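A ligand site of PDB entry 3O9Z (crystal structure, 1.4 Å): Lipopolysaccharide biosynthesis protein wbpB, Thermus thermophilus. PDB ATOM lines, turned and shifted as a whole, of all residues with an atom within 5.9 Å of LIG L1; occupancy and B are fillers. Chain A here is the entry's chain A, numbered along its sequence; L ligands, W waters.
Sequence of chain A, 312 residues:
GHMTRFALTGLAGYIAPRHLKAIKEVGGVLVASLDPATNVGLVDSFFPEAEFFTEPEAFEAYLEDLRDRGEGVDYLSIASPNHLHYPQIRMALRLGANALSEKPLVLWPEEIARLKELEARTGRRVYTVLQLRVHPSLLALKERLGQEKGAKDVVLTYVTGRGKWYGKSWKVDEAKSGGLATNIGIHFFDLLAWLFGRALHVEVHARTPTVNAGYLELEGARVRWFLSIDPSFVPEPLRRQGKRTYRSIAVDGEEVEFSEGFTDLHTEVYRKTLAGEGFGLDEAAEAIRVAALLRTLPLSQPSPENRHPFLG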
ATOM      1  N   LYS A 103      26.516  15.086  28.202  1.00  0.00           N
ATOM      2  CA  LYS A 103      26.085  14.865  29.583  1.00  0.00           C
ATOM      3  C   LYS A 103      26.302  13.412  30.004  1.00  0.00           C
ATOM      4  O   LYS A 103      26.402  12.507  29.149  1.00  0.00           O
ATOM      5  CB  LYS A 103      24.615  15.300  29.804  1.00  0.00           C
ATOM      6  CG  LYS A 103      23.607  14.881  28.726  1.00  0.00           C
ATOM      7  CD  LYS A 103      23.481  13.369  28.414  1.00  0.00           C
ATOM      8  CE  LYS A 103      22.993  12.538  29.602  1.00  0.00           C
ATOM      9  NZ  LYS A 103      22.940  11.100  29.084  1.00  0.00           N
ATOM     10  N   GLN A 131      20.773  19.767  26.442  1.00  0.00           N
ATOM     11  CA  GLN A 131      19.853  20.387  25.504  1.00  0.00           C
ATOM     12  C   GLN A 131      18.548  20.835  26.101  1.00  0.00           C
ATOM     13  O   GLN A 131      17.849  21.603  25.446  1.00  0.00           O
ATOM     14  CB  GLN A 131      19.627  19.473  24.294  1.00  0.00           C
ATOM     15  CG  GLN A 131      18.715  18.291  24.528  1.00  0.00           C
ATOM     16  CD  GLN A 131      19.435  16.958  24.699  1.00  0.00           C
ATOM     17  OE1 GLN A 131      18.920  15.915  24.236  1.00  0.00           O
ATOM     18  NE2 GLN A 131      20.618  16.963  25.282  1.00  0.00           N
ATOM     19  N   TYR A 158       9.690  11.224  34.246  1.00  0.00           N
ATOM     20  CA  TYR A 158      10.673  11.112  33.157  1.00  0.00           C
ATOM     21  C   TYR A 158      10.768   9.641  32.780  1.00  0.00           C
ATOM     22  O   TYR A 158      11.449   8.855  33.474  1.00  0.00           O
ATOM     23  CB  TYR A 158      12.029  11.673  33.629  1.00  0.00           C
ATOM     24  CG  TYR A 158      12.938  12.065  32.497  1.00  0.00           C
ATOM     25  CD1 TYR A 158      13.652  11.109  31.759  1.00  0.00           C
ATOM     26  CD2 TYR A 158      13.051  13.400  32.127  1.00  0.00           C
ATOM     27  CE1 TYR A 158      14.494  11.515  30.715  1.00  0.00           C
ATOM     28  CE2 TYR A 158      13.853  13.806  31.075  1.00  0.00           C
ATOM     29  CZ  TYR A 158      14.584  12.873  30.376  1.00  0.00           C
ATOM     30  OH  TYR A 158      15.402  13.246  29.326  1.00  0.00           O
ATOM     31  N   THR A 160      11.609   7.059  29.614  1.00  0.00           N
ATOM     32  CA  THR A 160      12.154   6.984  28.269  1.00  0.00           C
ATOM     33  C   THR A 160      12.555   5.536  27.979  1.00  0.00           C
ATOM     34  O   THR A 160      13.513   5.011  28.577  1.00  0.00           O
ATOM     35  CB  THR A 160      13.275   8.016  28.051  1.00  0.00           C
ATOM     36  OG1 THR A 160      13.738   7.905  26.692  1.00  0.00           O
ATOM     37  CG2 THR A 160      14.444   7.783  29.006  1.00  0.00           C
ATOM     38  N   ARG A 162      13.803   1.886  27.027  1.00  0.00           N
ATOM     39  CA  ARG A 162      15.062   1.338  26.475  1.00  0.00           C
ATOM     40  C   ARG A 162      14.886  -0.158  26.251  1.00  0.00           C
ATOM     41  O   ARG A 162      14.455  -0.919  27.142  1.00  0.00           O
ATOM     42  CB  ARG A 162      16.244   1.563  27.424  1.00  0.00           C
ATOM     43  CG  ARG A 162      16.638   3.025  27.534  1.00  0.00           C
ATOM     44  CD  ARG A 162      17.306   3.559  26.255  1.00  0.00           C
ATOM     45  NE  ARG A 162      17.733   4.935  26.424  1.00  0.00           N
ATOM     46  CZ  ARG A 162      16.928   5.988  26.330  1.00  0.00           C
ATOM     47  NH1 ARG A 162      15.625   5.822  26.154  1.00  0.00           N
ATOM     48  NH2 ARG A 162      17.436   7.225  26.473  1.00  0.00           N
ATOM     49  N   TYR A 166      20.247  -2.169  26.201  1.00  0.00           N
ATOM     50  CA  TYR A 166      20.743  -1.220  27.231  1.00  0.00           C
ATOM     51  C   TYR A 166      21.335  -1.987  28.413  1.00  0.00           C
ATOM     52  O   TYR A 166      22.420  -1.618  28.916  1.00  0.00           O
ATOM     53  CB  TYR A 166      19.580  -0.295  27.590  1.00  0.00           C
ATOM     54  CG  TYR A 166      19.892   0.829  28.532  1.00  0.00           C
ATOM     55  CD1 TYR A 166      20.104   2.111  28.039  1.00  0.00           C
ATOM     56  CD2 TYR A 166      19.877   0.644  29.909  1.00  0.00           C
ATOM     57  CE1 TYR A 166      20.364   3.179  28.914  1.00  0.00           C
ATOM     58  CE2 TYR A 166      20.118   1.714  30.807  1.00  0.00           C
ATOM     59  CZ  TYR A 166      20.365   2.930  30.283  1.00  0.00           C
ATOM     60  OH  TYR A 166      20.605   4.033  31.126  1.00  0.00           O
ATOM     61  N   LYS A 171      26.027   1.356  29.818  1.00  0.00           N
ATOM     62  CA  LYS A 171      25.027   2.198  30.465  1.00  0.00           C
ATOM     63  C   LYS A 171      24.552   1.708  31.800  1.00  0.00           C
ATOM     64  O   LYS A 171      24.095   2.503  32.648  1.00  0.00           O
ATOM     65  CB  LYS A 171      23.897   2.562  29.483  1.00  0.00           C
ATOM     66  CG  LYS A 171      24.416   3.395  28.281  1.00  0.00           C
ATOM     67  CD  LYS A 171      23.578   3.164  27.033  1.00  0.00           C
ATOM     68  CE  LYS A 171      24.102   3.924  25.827  1.00  0.00           C
ATOM     69  NZ  LYS A 171      23.580   5.344  25.819  1.00  0.00           N
ATOM     70  N   ASN A 183      22.933   8.629  34.370  1.00  0.00           N
ATOM     71  CA  ASN A 183      22.970   8.471  32.928  1.00  0.00           C
ATOM     72  C   ASN A 183      21.744   9.017  32.260  1.00  0.00           C
ATOM     73  O   ASN A 183      21.894   9.681  31.255  1.00  0.00           O
ATOM     74  CB  ASN A 183      23.163   7.007  32.555  1.00  0.00           C
ATOM     75  CG  ASN A 183      23.443   6.842  31.083  1.00  0.00           C
ATOM     76  OD1 ASN A 183      24.333   7.508  30.548  1.00  0.00           O
ATOM     77  ND2 ASN A 183      22.628   6.026  30.391  1.00  0.00           N
ATOM     78  N   ILE A 184      20.559   8.747  32.807  1.00  0.00           N
ATOM     79  CA  ILE A 184      19.364   9.320  32.217  1.00  0.00           C
ATOM     80  C   ILE A 184      18.927  10.523  33.056  1.00  0.00           C
ATOM     81  O   ILE A 184      18.614  11.553  32.502  1.00  0.00           O
ATOM     82  CB  ILE A 184      18.258   8.275  32.159  1.00  0.00           C
ATOM     83  CG1 ILE A 184      18.726   7.021  31.415  1.00  0.00           C
ATOM     84  CG2 ILE A 184      17.020   8.873  31.464  1.00  0.00           C
ATOM     85  CD1 ILE A 184      19.089   7.194  29.940  1.00  0.00           C
ATOM     86  N   HIS A 187      19.585  14.836  32.998  1.00  0.00           N
ATOM     87  CA  HIS A 187      18.817  15.799  32.232  1.00  0.00           C
ATOM     88  C   HIS A 187      17.860  16.538  33.158  1.00  0.00           C
ATOM     89  O   HIS A 187      17.788  17.763  33.085  1.00  0.00           O
ATOM     90  CB  HIS A 187      18.017  15.101  31.138  1.00  0.00           C
ATOM     91  CG  HIS A 187      18.803  14.776  29.909  1.00  0.00           C
ATOM     92  ND1 HIS A 187      19.301  15.741  29.048  1.00  0.00           N
ATOM     93  CD2 HIS A 187      19.131  13.577  29.371  1.00  0.00           C
ATOM     94  CE1 HIS A 187      19.902  15.146  28.034  1.00  0.00           C
ATOM     95  NE2 HIS A 187      19.840  13.834  28.210  1.00  0.00           N
ATOM     96  N   THR A 245       7.853   7.233  25.417  1.00  0.00           N
ATOM     97  CA  THR A 245       8.451   8.276  26.213  1.00  0.00           C
ATOM     98  C   THR A 245       7.354   9.170  26.787  1.00  0.00           C
ATOM     99  O   THR A 245       6.283   9.397  26.192  1.00  0.00           O
ATOM    100  CB  THR A 245       9.415   9.170  25.438  1.00  0.00           C
ATOM    101  OG1 THR A 245       8.692   9.962  24.498  1.00  0.00           O
ATOM    102  CG2 THR A 245      10.493   8.323  24.700  1.00  0.00           C
ATOM    103  N   ARG A 247       7.963  12.774  29.149  1.00  0.00           N
ATOM    104  CA  ARG A 247       8.878  13.664  29.855  1.00  0.00           C
ATOM    105  C   ARG A 247       8.136  14.917  30.249  1.00  0.00           C
ATOM    106  O   ARG A 247       7.811  15.750  29.382  1.00  0.00           O
ATOM    107  CB  ARG A 247      10.124  14.007  29.027  1.00  0.00           C
ATOM    108  CG  ARG A 247      10.939  12.808  28.548  1.00  0.00           C
ATOM    109  CD  ARG A 247      12.095  13.347  27.669  1.00  0.00           C
ATOM    110  NE  ARG A 247      12.848  12.308  26.969  1.00  0.00           N
ATOM    111  CZ  ARG A 247      12.632  11.925  25.720  1.00  0.00           C
ATOM    112  NH1 ARG A 247      11.567  12.409  25.061  1.00  0.00           N
ATOM    113  NH2 ARG A 247      13.435  11.045  25.131  1.00  0.00           N
ATOM    114  N   PHE A 262      13.091  17.023  21.504  1.00  0.00           N
ATOM    115  CA  PHE A 262      14.197  16.560  22.366  1.00  0.00           C
ATOM    116  C   PHE A 262      15.471  16.106  21.639  1.00  0.00           C
ATOM    117  O   PHE A 262      16.582  16.351  22.120  1.00  0.00           O
ATOM    118  CB  PHE A 262      13.692  15.424  23.285  1.00  0.00           C
ATOM    119  CG  PHE A 262      14.681  14.987  24.336  1.00  0.00           C
ATOM    120  CD1 PHE A 262      14.817  15.695  25.522  1.00  0.00           C
ATOM    121  CD2 PHE A 262      15.525  13.889  24.150  1.00  0.00           C
ATOM    122  CE1 PHE A 262      15.752  15.307  26.485  1.00  0.00           C
ATOM    123  CE2 PHE A 262      16.449  13.492  25.117  1.00  0.00           C
ATOM    124  CZ  PHE A 262      16.549  14.169  26.314  1.00  0.00           C
HETATM  125  C1  LIG L   1      20.672   9.022  26.977  1.00  0.00           C
HETATM  126  O1  LIG L   1      20.106   8.012  26.496  1.00  0.00           O
HETATM  127  O2  LIG L   1      21.832   8.980  27.400  1.00  0.00           O
HETATM  128  C2  LIG L   1      20.068  10.334  26.958  1.00  0.00           C
HETATM  129  O3  LIG L   1      20.691  11.285  27.427  1.00  0.00           O
HETATM  130  C3  LIG L   1      18.683  10.535  26.388  1.00  0.00           C
HETATM  131  C4  LIG L   1      17.693  10.470  27.547  1.00  0.00           C
HETATM  132  C5  LIG L   1      16.243  10.468  27.105  1.00  0.00           C
HETATM  133  O4  LIG L   1      15.884   9.717  26.179  1.00  0.00           O
HETATM  134  O5  LIG L   1      15.449  11.221  27.670  1.00  0.00           O
HETATM  135  P1  LG2 L   2      27.156   4.300  22.604  1.00  0.00           P
HETATM  136  O1  LG2 L   2      26.225   4.176  21.455  1.00  0.00           O
HETATM  137  O2  LG2 L   2      27.474   3.111  23.515  1.00  0.00           O
HETATM  138  O3  LG2 L   2      28.464   4.840  21.894  1.00  0.00           O
HETATM  139  C1  LG2 L   2      29.566   4.977  22.742  1.00  0.00           C
HETATM  140  C2  LG2 L   2      30.827   5.064  21.850  1.00  0.00           C
HETATM  141  O4  LG2 L   2      31.996   5.397  22.650  1.00  0.00           O
HETATM  142  C3  LG2 L   2      31.125   3.657  21.273  1.00  0.00           C
HETATM  143  O5  LG2 L   2      31.216   3.688  19.825  1.00  0.00           O
HETATM  144  C4  LG2 L   2      32.422   3.211  21.956  1.00  0.00           C
HETATM  145  O6  LG2 L   2      33.270   2.358  21.168  1.00  0.00           O
HETATM  146  C5  LG2 L   2      33.073   4.617  22.117  1.00  0.00           C
HETATM  147  N1  LG2 L   2      34.170   4.570  23.116  1.00  0.00           N
HETATM  148  C6  LG2 L   2      34.504   3.723  24.137  1.00  0.00           C
HETATM  149  N2  LG2 L   2      35.646   4.106  24.714  1.00  0.00           N
HETATM  150  C7  LG2 L   2      36.128   5.176  24.004  1.00  0.00           C
HETATM  151  C8  LG2 L   2      37.297   6.019  24.102  1.00  0.00           C
HETATM  152  N3  LG2 L   2      38.262   5.755  25.043  1.00  0.00           N
HETATM  153  N4  LG2 L   2      37.317   6.987  23.191  1.00  0.00           N
HETATM  154  C9  LG2 L   2      36.445   7.301  22.247  1.00  0.00           C
HETATM  155  N5  LG2 L   2      35.345   6.514  22.125  1.00  0.00           N
HETATM  156  C10 LG2 L   2      35.203   5.515  23.001  1.00  0.00           C
HETATM  157  O7  LG2 L   2      26.639   5.482  23.548  1.00  0.00           O
HETATM  158  P2  LG2 L   2      25.888   6.813  23.233  1.00  0.00           P
HETATM  159  O8  LG2 L   2      24.395   6.616  23.501  1.00  0.00           O
HETATM  160  O9  LG2 L   2      26.312   7.362  21.903  1.00  0.00           O
HETATM  161  O10 LG2 L   2      26.314   7.751  24.454  1.00  0.00           O
HETATM  162  C11 LG2 L   2      27.511   8.456  24.216  1.00  0.00           C
HETATM  163  C12 LG2 L   2      27.511   9.634  25.218  1.00  0.00           C
HETATM  164  O11 LG2 L   2      26.460  10.512  24.756  1.00  0.00           O
HETATM  165  C13 LG2 L   2      27.216   9.288  26.683  1.00  0.00           C
HETATM  166  O12 LG2 L   2      27.933  10.283  27.478  1.00  0.00           O
HETATM  167  C14 LG2 L   2      25.720   9.609  26.772  1.00  0.00           C
HETATM  168  O13 LG2 L   2      25.328   9.997  28.083  1.00  0.00           O
HETATM  169  C15 LG2 L   2      25.470  10.734  25.779  1.00  0.00           C
HETATM  170  N6  LG2 L   2      24.111  10.756  25.241  1.00  0.00           N
HETATM  171  C16 LG2 L   2      23.440  11.886  25.230  1.00  0.00           C
HETATM  172  C17 LG2 L   2      22.156  12.038  24.748  1.00  0.00           C
HETATM  173  C18 LG2 L   2      21.538  13.369  24.887  1.00  0.00           C
HETATM  174  O14 LG2 L   2      22.231  14.403  25.003  1.00  0.00           O
HETATM  175  N7  LG2 L   2      20.221  13.384  24.754  1.00  0.00           N
HETATM  176  C19 LG2 L   2      21.551  10.894  24.202  1.00  0.00           C
HETATM  177  C20 LG2 L   2      22.324   9.737  24.145  1.00  0.00           C
HETATM  178  C21 LG2 L   2      23.617   9.664  24.656  1.00  0.00           C
HETATM  179  O   HOH W   1      20.658   5.465  25.958  1.00  0.00           O
HETATM  180  O   HOH W   2      23.726   7.133  27.904  1.00  0.00           O
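Water W1 lies within hydrogen-bond range of an oxygen (O1) of LIG L1 (2.7 Å), the side-chain amino group (NZ) of Lys 171 (2.9 Å) and the guanidinium group (NE) of Arg 162 (3.0 Å).
Water W2 lies within hydrogen-bond range of an oxygen (O2) of LIG L1 (2.7 Å), the side-chain amide oxygen of Asn 183 (2.7 Å), the side-chain amino group of Lys 171 (2.8 Å) and an oxygen (O13) of LG2 L2 (3.3 Å).
The guanidinium group of Arg 162 sits at hydrogen-bond distance from the side-chain hydroxyl of Thr 160 (2.9 Å).
The backbone carbonyl oxygen (O) of Asn 183 is in hydrogen-bond range of the side-chain amino group (NZ) of Lys 103 (2.8 Å).
O of Phe 262 sits close to OE1 of Gln 131.
The side-chain hydroxyl (OH) of Tyr 166 sits at hydrogen-bond distance from the side-chain amide nitrogen (ND2) of Asn 183, at 2.9 Å.
An oxygen (O5) of LIG L1 sits at hydrogen-bond distance from the side-chain hydroxyl (OH) of Tyr 158.
An oxygen (O1) of LIG L1 is in salt-bridge range of the guanidinium group of Arg 162 (2.8 Å).
A ring nitrogen (NE2) of His 187 sits at hydrogen-bond distance from an oxygen (O3) of LIG L1, 2.8 Å away.
An oxygen (O2) of LIG L1 is in salt-bridge range of the side-chain amino group of Lys 103 (2.9 Å).
The side-chain hydroxyl (OG1) of Thr 160 sits at hydrogen-bond distance from an oxygen (O4) of LIG L1 (2.9 Å).
An oxygen (O5) of LIG L1 is in salt-bridge range of the guanidinium group (NE) of Arg 247.
An oxygen (O13) of LG2 L2 lies within hydrogen-bond range of the backbone carbonyl oxygen (O) of Lys 103.
NZ of Lys 103 sits at hydrogen-bond distance from O13 of LG2 L2 (2.8 Å).
NZ of Lys 171 lies within salt-bridge range of O8 of LG2 L2 (2.8 Å).
OE1 of Gln 131 lies within hydrogen-bond range of N7 of LG2 L2 (2.9 Å).
O of Asn 183 touches O2 of LIG L1, at 3.9 Å.
Ile 184 touches LIG L1 (CD1 to O1, 3.7 Å).
CZ of Phe 262 touches O5 of LIG L1, 3.4 Å away.
Hydrophobic or aromatic side chains that line LIG L1: Tyr 158, Ile 184, His 187 and Phe 262.
Nine residues have an atom within 4 Å of LIG L1: Lys 103, Tyr 158, Thr 160, Arg 162, Asn 183, Ile 184, His 187, Arg 247 and Phe 262.
A nitrogen (N7) of LG2 L2 lies close to an oxygen (O3) of LIG L1 (3.4 Å).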
